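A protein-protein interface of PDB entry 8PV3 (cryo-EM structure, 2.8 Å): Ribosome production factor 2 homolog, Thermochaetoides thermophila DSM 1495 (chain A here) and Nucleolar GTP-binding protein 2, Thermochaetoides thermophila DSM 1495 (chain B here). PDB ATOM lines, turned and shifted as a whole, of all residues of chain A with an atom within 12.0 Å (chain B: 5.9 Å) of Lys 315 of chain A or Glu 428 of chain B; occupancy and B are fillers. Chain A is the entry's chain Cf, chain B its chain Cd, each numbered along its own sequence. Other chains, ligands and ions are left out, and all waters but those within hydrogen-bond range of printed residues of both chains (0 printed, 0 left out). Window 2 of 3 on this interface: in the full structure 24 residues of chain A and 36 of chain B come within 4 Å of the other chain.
The backbone carbonyl oxygen (O) of Gly 316 of chain A sits at hydrogen-bond distance from the guanidinium group (NE) of Arg 425 of chain B, at 3.3 Å.
The side-chain carboxylate (OE1) of Glu 428 of chain B lies within salt-bridge range of the side-chain amino group (NZ) of Lys 315 of chain A (2.6 Å).
NE of Arg 319 of chain A lies close to NH1 of Arg 425 of chain B (3.3 Å).
The side-chain carboxylate of Glu 428 of chain B lies within salt-bridge range of the side-chain amino group of Lys 445 of chain B (3.8 Å).
Lys 472 of chain B touches Met 314 of chain A.
Lys 315 of chain A touches Arg 425 of chain B (O to O, 3.7 Å).
CD of Lys 315 of chain A touches O of Thr 426 of chain B (3.8 Å).
Gly 316 of chain A touches Thr 426 of chain B (CA to OG1, 3.5 Å).
Arg 425 of chain B touches Lys 318 of chain A (CG to O, 3.6 Å).
Of chain A, only Lys 315 comes within 4 Å of Glu 428 of chain B.
Of chain A, only Lys 315 (3.7 Å), Gly 316 (3.3 Å), Lys 318 (3.6 Å) and Arg 319 (3.2 Å) come within 4 Å of Arg 425 of chain B.
Thr 426 of chain B touches just these residues of chain A: Lys 315 and Gly 316.
No residue of chain A comes within 4 Å of Leu 429 of chain B.
Printed residues of chain B within 4 Å of Met 314 of chain A: Lys 472.
Printed residues of chain B within 4 Å of Lys 318 of chain A: Arg 425 (3.6 Å).
Of the printed residues of chain A, Lys 472 of chain B touches Met 314 (3.5 Å).
Of the printed residues of chain B, Gly 316 of chain A touches Arg 425 and Thr 426.
The nearest residue of chain B that does not touch Lys 315 of chain A is Lys 472 of chain B (5.1 Å).
The nearest printed residue of chain B that does not touch Lys 318 of chain A is Thr 426 of chain B (6.9 Å).
Of the 10 printed residues of chain B, 4 touch a printed residue of chain A.
Hydrophobic or aromatic side chains of chain A that line the printed part of chain B: Met 314.
Along chain A the printed residues that touch a printed residue of chain B span positions 314 to 319.
Among the printed residues, Asp or Glu carboxylates within 4 Å of a Lys or Arg side-chain nitrogen of the other chain: Lys 315 of chain A with Glu 428 of chain B (2.6 Å).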
ATOM      1  N   THR A 311      25.628  -4.270 -14.658  1.00  0.00           N
ATOM      2  CA  THR A 311      25.653  -4.538 -13.229  1.00  0.00           C
ATOM      3  C   THR A 311      24.675  -5.656 -12.884  1.00  0.00           C
ATOM      4  O   THR A 311      23.854  -6.080 -13.701  1.00  0.00           O
ATOM      5  CB  THR A 311      25.308  -3.279 -12.437  1.00  0.00           C
ATOM      6  OG1 THR A 311      24.143  -2.665 -13.000  1.00  0.00           O
ATOM      7  CG2 THR A 311      26.460  -2.295 -12.486  1.00  0.00           C
ATOM      8  N   ARG A 312      24.771  -6.142 -11.650  1.00  0.00           N
ATOM      9  CA  ARG A 312      23.908  -7.232 -11.228  1.00  0.00           C
ATOM     10  C   ARG A 312      22.496  -6.722 -10.977  1.00  0.00           C
ATOM     11  O   ARG A 312      22.295  -5.734 -10.264  1.00  0.00           O
ATOM     12  CB  ARG A 312      24.466  -7.897  -9.973  1.00  0.00           C
ATOM     13  CG  ARG A 312      23.776  -9.199  -9.633  1.00  0.00           C
ATOM     14  CD  ARG A 312      24.499  -9.953  -8.543  1.00  0.00           C
ATOM     15  NE  ARG A 312      23.927 -11.279  -8.352  1.00  0.00           N
ATOM     16  CZ  ARG A 312      24.282 -12.355  -9.040  1.00  0.00           C
ATOM     17  NH1 ARG A 312      25.220 -12.301  -9.971  1.00  0.00           N
ATOM     18  NH2 ARG A 312      23.682 -13.514  -8.787  1.00  0.00           N
ATOM     19  N   LYS A 313      21.514  -7.404 -11.565  1.00  0.00           N
ATOM     20  CA  LYS A 313      20.110  -7.015 -11.445  1.00  0.00           C
ATOM     21  C   LYS A 313      19.556  -7.588 -10.142  1.00  0.00           C
ATOM     22  O   LYS A 313      18.846  -8.594 -10.104  1.00  0.00           O
ATOM     23  CB  LYS A 313      19.315  -7.485 -12.653  1.00  0.00           C
ATOM     24  CG  LYS A 313      19.968  -7.179 -13.994  1.00  0.00           C
ATOM     25  CD  LYS A 313      20.286  -5.701 -14.153  1.00  0.00           C
ATOM     26  CE  LYS A 313      21.075  -5.450 -15.425  1.00  0.00           C
ATOM     27  NZ  LYS A 313      21.637  -4.075 -15.467  1.00  0.00           N
ATOM     28  N   MET A 314      19.902  -6.915  -9.050  1.00  0.00           N
ATOM     29  CA  MET A 314      19.588  -7.424  -7.726  1.00  0.00           C
ATOM     30  C   MET A 314      18.181  -7.014  -7.307  1.00  0.00           C
ATOM     31  O   MET A 314      17.612  -6.046  -7.816  1.00  0.00           O
ATOM     32  CB  MET A 314      20.627  -6.932  -6.724  1.00  0.00           C
ATOM     33  CG  MET A 314      21.918  -7.734  -6.806  1.00  0.00           C
ATOM     34  SD  MET A 314      23.286  -7.076  -5.845  1.00  0.00           S
ATOM     35  CE  MET A 314      22.403  -6.370  -4.473  1.00  0.00           C
ATOM     36  N   LYS A 315      17.622  -7.783  -6.368  1.00  0.00           N
ATOM     37  CA  LYS A 315      16.208  -7.660  -6.022  1.00  0.00           C
ATOM     38  C   LYS A 315      15.904  -6.328  -5.343  1.00  0.00           C
ATOM     39  O   LYS A 315      14.814  -5.771  -5.512  1.00  0.00           O
ATOM     40  CB  LYS A 315      15.802  -8.830  -5.127  1.00  0.00           C
ATOM     41  CG  LYS A 315      14.319  -8.932  -4.831  1.00  0.00           C
ATOM     42  CD  LYS A 315      14.047 -10.045  -3.836  1.00  0.00           C
ATOM     43  CE  LYS A 315      12.567 -10.363  -3.751  1.00  0.00           C
ATOM     44  NZ  LYS A 315      12.279 -11.363  -2.687  1.00  0.00           N
ATOM     45  N   GLY A 316      16.859  -5.797  -4.576  1.00  0.00           N
ATOM     46  CA  GLY A 316      16.643  -4.532  -3.898  1.00  0.00           C
ATOM     47  C   GLY A 316      16.671  -3.325  -4.811  1.00  0.00           C
ATOM     48  O   GLY A 316      16.189  -2.258  -4.421  1.00  0.00           O
ATOM     49  N   LEU A 317      17.224  -3.467  -6.012  1.00  0.00           N
ATOM     50  CA  LEU A 317      17.314  -2.372  -6.967  1.00  0.00           C
ATOM     51  C   LEU A 317      16.129  -2.307  -7.917  1.00  0.00           C
ATOM     52  O   LEU A 317      16.069  -1.393  -8.745  1.00  0.00           O
ATOM     53  CB  LEU A 317      18.608  -2.482  -7.778  1.00  0.00           C
ATOM     54  CG  LEU A 317      19.914  -2.337  -7.006  1.00  0.00           C
ATOM     55  CD1 LEU A 317      21.095  -2.516  -7.936  1.00  0.00           C
ATOM     56  CD2 LEU A 317      19.966  -0.985  -6.323  1.00  0.00           C
ATOM     57  N   LYS A 318      15.191  -3.244  -7.825  1.00  0.00           N
ATOM     58  CA  LYS A 318      14.044  -3.294  -8.721  1.00  0.00           C
ATOM     59  C   LYS A 318      12.849  -2.638  -8.041  1.00  0.00           C
ATOM     60  O   LYS A 318      12.513  -2.979  -6.902  1.00  0.00           O
ATOM     61  CB  LYS A 318      13.722  -4.737  -9.110  1.00  0.00           C
ATOM     62  CG  LYS A 318      14.852  -5.438  -9.845  1.00  0.00           C
ATOM     63  CD  LYS A 318      14.513  -6.889 -10.137  1.00  0.00           C
ATOM     64  CE  LYS A 318      15.608  -7.553 -10.956  1.00  0.00           C
ATOM     65  NZ  LYS A 318      15.322  -8.991 -11.212  1.00  0.00           N
ATOM     66  N   ARG A 319      12.217  -1.700  -8.739  1.00  0.00           N
ATOM     67  CA  ARG A 319      11.061  -0.984  -8.212  1.00  0.00           C
ATOM     68  C   ARG A 319       9.839  -1.892  -8.116  1.00  0.00           C
ATOM     69  O   ARG A 319       9.567  -2.680  -9.022  1.00  0.00           O
ATOM     70  CB  ARG A 319      10.745   0.230  -9.089  1.00  0.00           C
ATOM     71  CG  ARG A 319       9.536   1.042  -8.643  1.00  0.00           C
ATOM     72  CD  ARG A 319       9.849   1.929  -7.444  1.00  0.00           C
ATOM     73  NE  ARG A 319       9.524   1.287  -6.176  1.00  0.00           N
ATOM     74  CZ  ARG A 319       9.841   1.779  -4.986  1.00  0.00           C
ATOM     75  NH1 ARG A 319      10.495   2.923  -4.863  1.00  0.00           N
ATOM     76  NH2 ARG A 319       9.494   1.106  -3.893  1.00  0.00           N
ATOM     77  N   MET B 423      16.672  -2.065   1.639  1.00  0.00           N
ATOM     78  CA  MET B 423      16.241  -3.136   2.532  1.00  0.00           C
ATOM     79  C   MET B 423      14.756  -3.440   2.354  1.00  0.00           C
ATOM     80  O   MET B 423      14.333  -4.601   2.439  1.00  0.00           O
ATOM     81  CB  MET B 423      16.546  -2.757   3.980  1.00  0.00           C
ATOM     82  CG  MET B 423      17.917  -3.197   4.456  1.00  0.00           C
ATOM     83  SD  MET B 423      17.889  -4.820   5.233  1.00  0.00           S
ATOM     84  CE  MET B 423      19.618  -5.027   5.638  1.00  0.00           C
ATOM     85  N   GLU B 424      13.952  -2.400   2.102  1.00  0.00           N
ATOM     86  CA  GLU B 424      12.517  -2.595   1.895  1.00  0.00           C
ATOM     87  C   GLU B 424      12.225  -3.438   0.655  1.00  0.00           C
ATOM     88  O   GLU B 424      11.448  -4.396   0.728  1.00  0.00           O
ATOM     89  CB  GLU B 424      11.806  -1.245   1.807  1.00  0.00           C
ATOM     90  CG  GLU B 424      11.958  -0.383   3.045  1.00  0.00           C
ATOM     91  CD  GLU B 424      10.771   0.529   3.268  1.00  0.00           C
ATOM     92  OE1 GLU B 424      10.910   1.517   4.020  1.00  0.00           O
ATOM     93  OE2 GLU B 424       9.706   0.273   2.671  1.00  0.00           O
ATOM     94  N   ARG B 425      12.834  -3.111  -0.489  1.00  0.00           N
ATOM     95  CA  ARG B 425      12.643  -3.966  -1.665  1.00  0.00           C
ATOM     96  C   ARG B 425      13.391  -5.290  -1.545  1.00  0.00           C
ATOM     97  O   ARG B 425      13.062  -6.250  -2.250  1.00  0.00           O
ATOM     98  CB  ARG B 425      13.036  -3.268  -2.973  1.00  0.00           C
ATOM     99  CG  ARG B 425      12.140  -2.129  -3.470  1.00  0.00           C
ATOM    100  CD  ARG B 425      12.508  -0.763  -2.960  1.00  0.00           C
ATOM    101  NE  ARG B 425      13.719  -0.254  -3.595  1.00  0.00           N
ATOM    102  CZ  ARG B 425      13.774   0.309  -4.794  1.00  0.00           C
ATOM    103  NH1 ARG B 425      12.694   0.440  -5.548  1.00  0.00           N
ATOM    104  NH2 ARG B 425      14.942   0.746  -5.253  1.00  0.00           N
ATOM    105  N   THR B 426      14.402  -5.370  -0.676  1.00  0.00           N
ATOM    106  CA  THR B 426      15.115  -6.634  -0.525  1.00  0.00           C
ATOM    107  C   THR B 426      14.278  -7.660   0.229  1.00  0.00           C
ATOM    108  O   THR B 426      14.183  -8.819  -0.189  1.00  0.00           O
ATOM    109  CB  THR B 426      16.448  -6.406   0.187  1.00  0.00           C
ATOM    110  OG1 THR B 426      17.205  -5.417  -0.519  1.00  0.00           O
ATOM    111  CG2 THR B 426      17.250  -7.695   0.235  1.00  0.00           C
ATOM    112  N   TYR B 427      13.650  -7.254   1.329  1.00  0.00           N
ATOM    113  CA  TYR B 427      12.934  -8.201   2.176  1.00  0.00           C
ATOM    114  C   TYR B 427      11.420  -8.043   2.126  1.00  0.00           C
ATOM    115  O   TYR B 427      10.721  -8.754   2.858  1.00  0.00           O
ATOM    116  CB  TYR B 427      13.431  -8.097   3.617  1.00  0.00           C
ATOM    117  CG  TYR B 427      14.845  -8.594   3.787  1.00  0.00           C
ATOM    118  CD1 TYR B 427      15.146  -9.941   3.646  1.00  0.00           C
ATOM    119  CD2 TYR B 427      15.881  -7.720   4.082  1.00  0.00           C
ATOM    120  CE1 TYR B 427      16.437 -10.404   3.795  1.00  0.00           C
ATOM    121  CE2 TYR B 427      17.175  -8.175   4.235  1.00  0.00           C
ATOM    122  CZ  TYR B 427      17.446  -9.516   4.090  1.00  0.00           C
ATOM    123  OH  TYR B 427      18.735  -9.970   4.241  1.00  0.00           O
ATOM    124  N   GLU B 428      10.902  -7.159   1.266  1.00  0.00           N
ATOM    125  CA  GLU B 428       9.466  -6.894   1.111  1.00  0.00           C
ATOM    126  C   GLU B 428       8.813  -6.554   2.451  1.00  0.00           C
ATOM    127  O   GLU B 428       7.728  -7.033   2.788  1.00  0.00           O
ATOM    128  CB  GLU B 428       8.760  -8.066   0.428  1.00  0.00           C
ATOM    129  CG  GLU B 428       9.278  -8.364  -0.968  1.00  0.00           C
ATOM    130  CD  GLU B 428       9.224  -9.837  -1.311  1.00  0.00           C
ATOM    131  OE1 GLU B 428      10.273 -10.510  -1.220  1.00  0.00           O
ATOM    132  OE2 GLU B 428       8.135 -10.326  -1.674  1.00  0.00           O
ATOM    133  N   LEU B 429       9.496  -5.712   3.221  1.00  0.00           N
ATOM    134  CA  LEU B 429       9.099  -5.407   4.586  1.00  0.00           C
ATOM    135  C   LEU B 429       9.313  -3.924   4.848  1.00  0.00           C
ATOM    136  O   LEU B 429      10.191  -3.292   4.257  1.00  0.00           O
ATOM    137  CB  LEU B 429       9.896  -6.255   5.585  1.00  0.00           C
ATOM    138  CG  LEU B 429       9.352  -6.426   6.998  1.00  0.00           C
ATOM    139  CD1 LEU B 429       8.184  -7.392   6.999  1.00  0.00           C
ATOM    140  CD2 LEU B 429      10.462  -6.917   7.903  1.00  0.00           C
ATOM    141  N   ARG B 430       8.498  -3.371   5.742  1.00  0.00           N
ATOM    142  CA  ARG B 430       8.587  -1.955   6.071  1.00  0.00           C
ATOM    143  C   ARG B 430       7.978  -1.712   7.443  1.00  0.00           C
ATOM    144  O   ARG B 430       7.247  -2.549   7.976  1.00  0.00           O
ATOM    145  CB  ARG B 430       7.887  -1.091   5.017  1.00  0.00           C
ATOM    146  CG  ARG B 430       6.390  -1.320   4.918  1.00  0.00           C
ATOM    147  CD  ARG B 430       5.759  -0.379   3.906  1.00  0.00           C
ATOM    148  NE  ARG B 430       6.620  -0.168   2.749  1.00  0.00           N
ATOM    149  CZ  ARG B 430       6.587  -0.906   1.647  1.00  0.00           C
ATOM    150  NH1 ARG B 430       5.740  -1.914   1.515  1.00  0.00           N
ATOM    151  NH2 ARG B 430       7.426  -0.627   0.653  1.00  0.00           N
ATOM    152  N   LYS B 445       7.841 -13.202   9.213  1.00  0.00           N
ATOM    153  CA  LYS B 445       7.460 -13.309   7.808  1.00  0.00           C
ATOM    154  C   LYS B 445       8.048 -14.558   7.164  1.00  0.00           C
ATOM    155  O   LYS B 445       7.337 -15.298   6.476  1.00  0.00           O
ATOM    156  CB  LYS B 445       7.907 -12.064   7.045  1.00  0.00           C
ATOM    157  CG  LYS B 445       7.646 -12.157   5.556  1.00  0.00           C
ATOM    158  CD  LYS B 445       8.478 -11.167   4.772  1.00  0.00           C
ATOM    159  CE  LYS B 445       8.367 -11.448   3.285  1.00  0.00           C
ATOM    160  NZ  LYS B 445       9.338 -10.654   2.492  1.00  0.00           N
ATOM    161  N   LYS B 472      23.903  -9.594  -1.978  1.00  0.00           N
ATOM    162  CA  LYS B 472      22.473  -9.724  -2.202  1.00  0.00           C
ATOM    163  C   LYS B 472      21.680  -8.504  -1.761  1.00  0.00           C
ATOM    164  O   LYS B 472      20.532  -8.350  -2.187  1.00  0.00           O
ATOM    165  CB  LYS B 472      21.929 -10.965  -1.482  1.00  0.00           C
ATOM    166  CG  LYS B 472      22.443 -12.273  -2.058  1.00  0.00           C
ATOM    167  CD  LYS B 472      21.804 -13.472  -1.383  1.00  0.00           C
ATOM    168  CE  LYS B 472      22.143 -14.759  -2.115  1.00  0.00           C
ATOM    169  NZ  LYS B 472      23.611 -14.945  -2.260  1.00  0.00           N
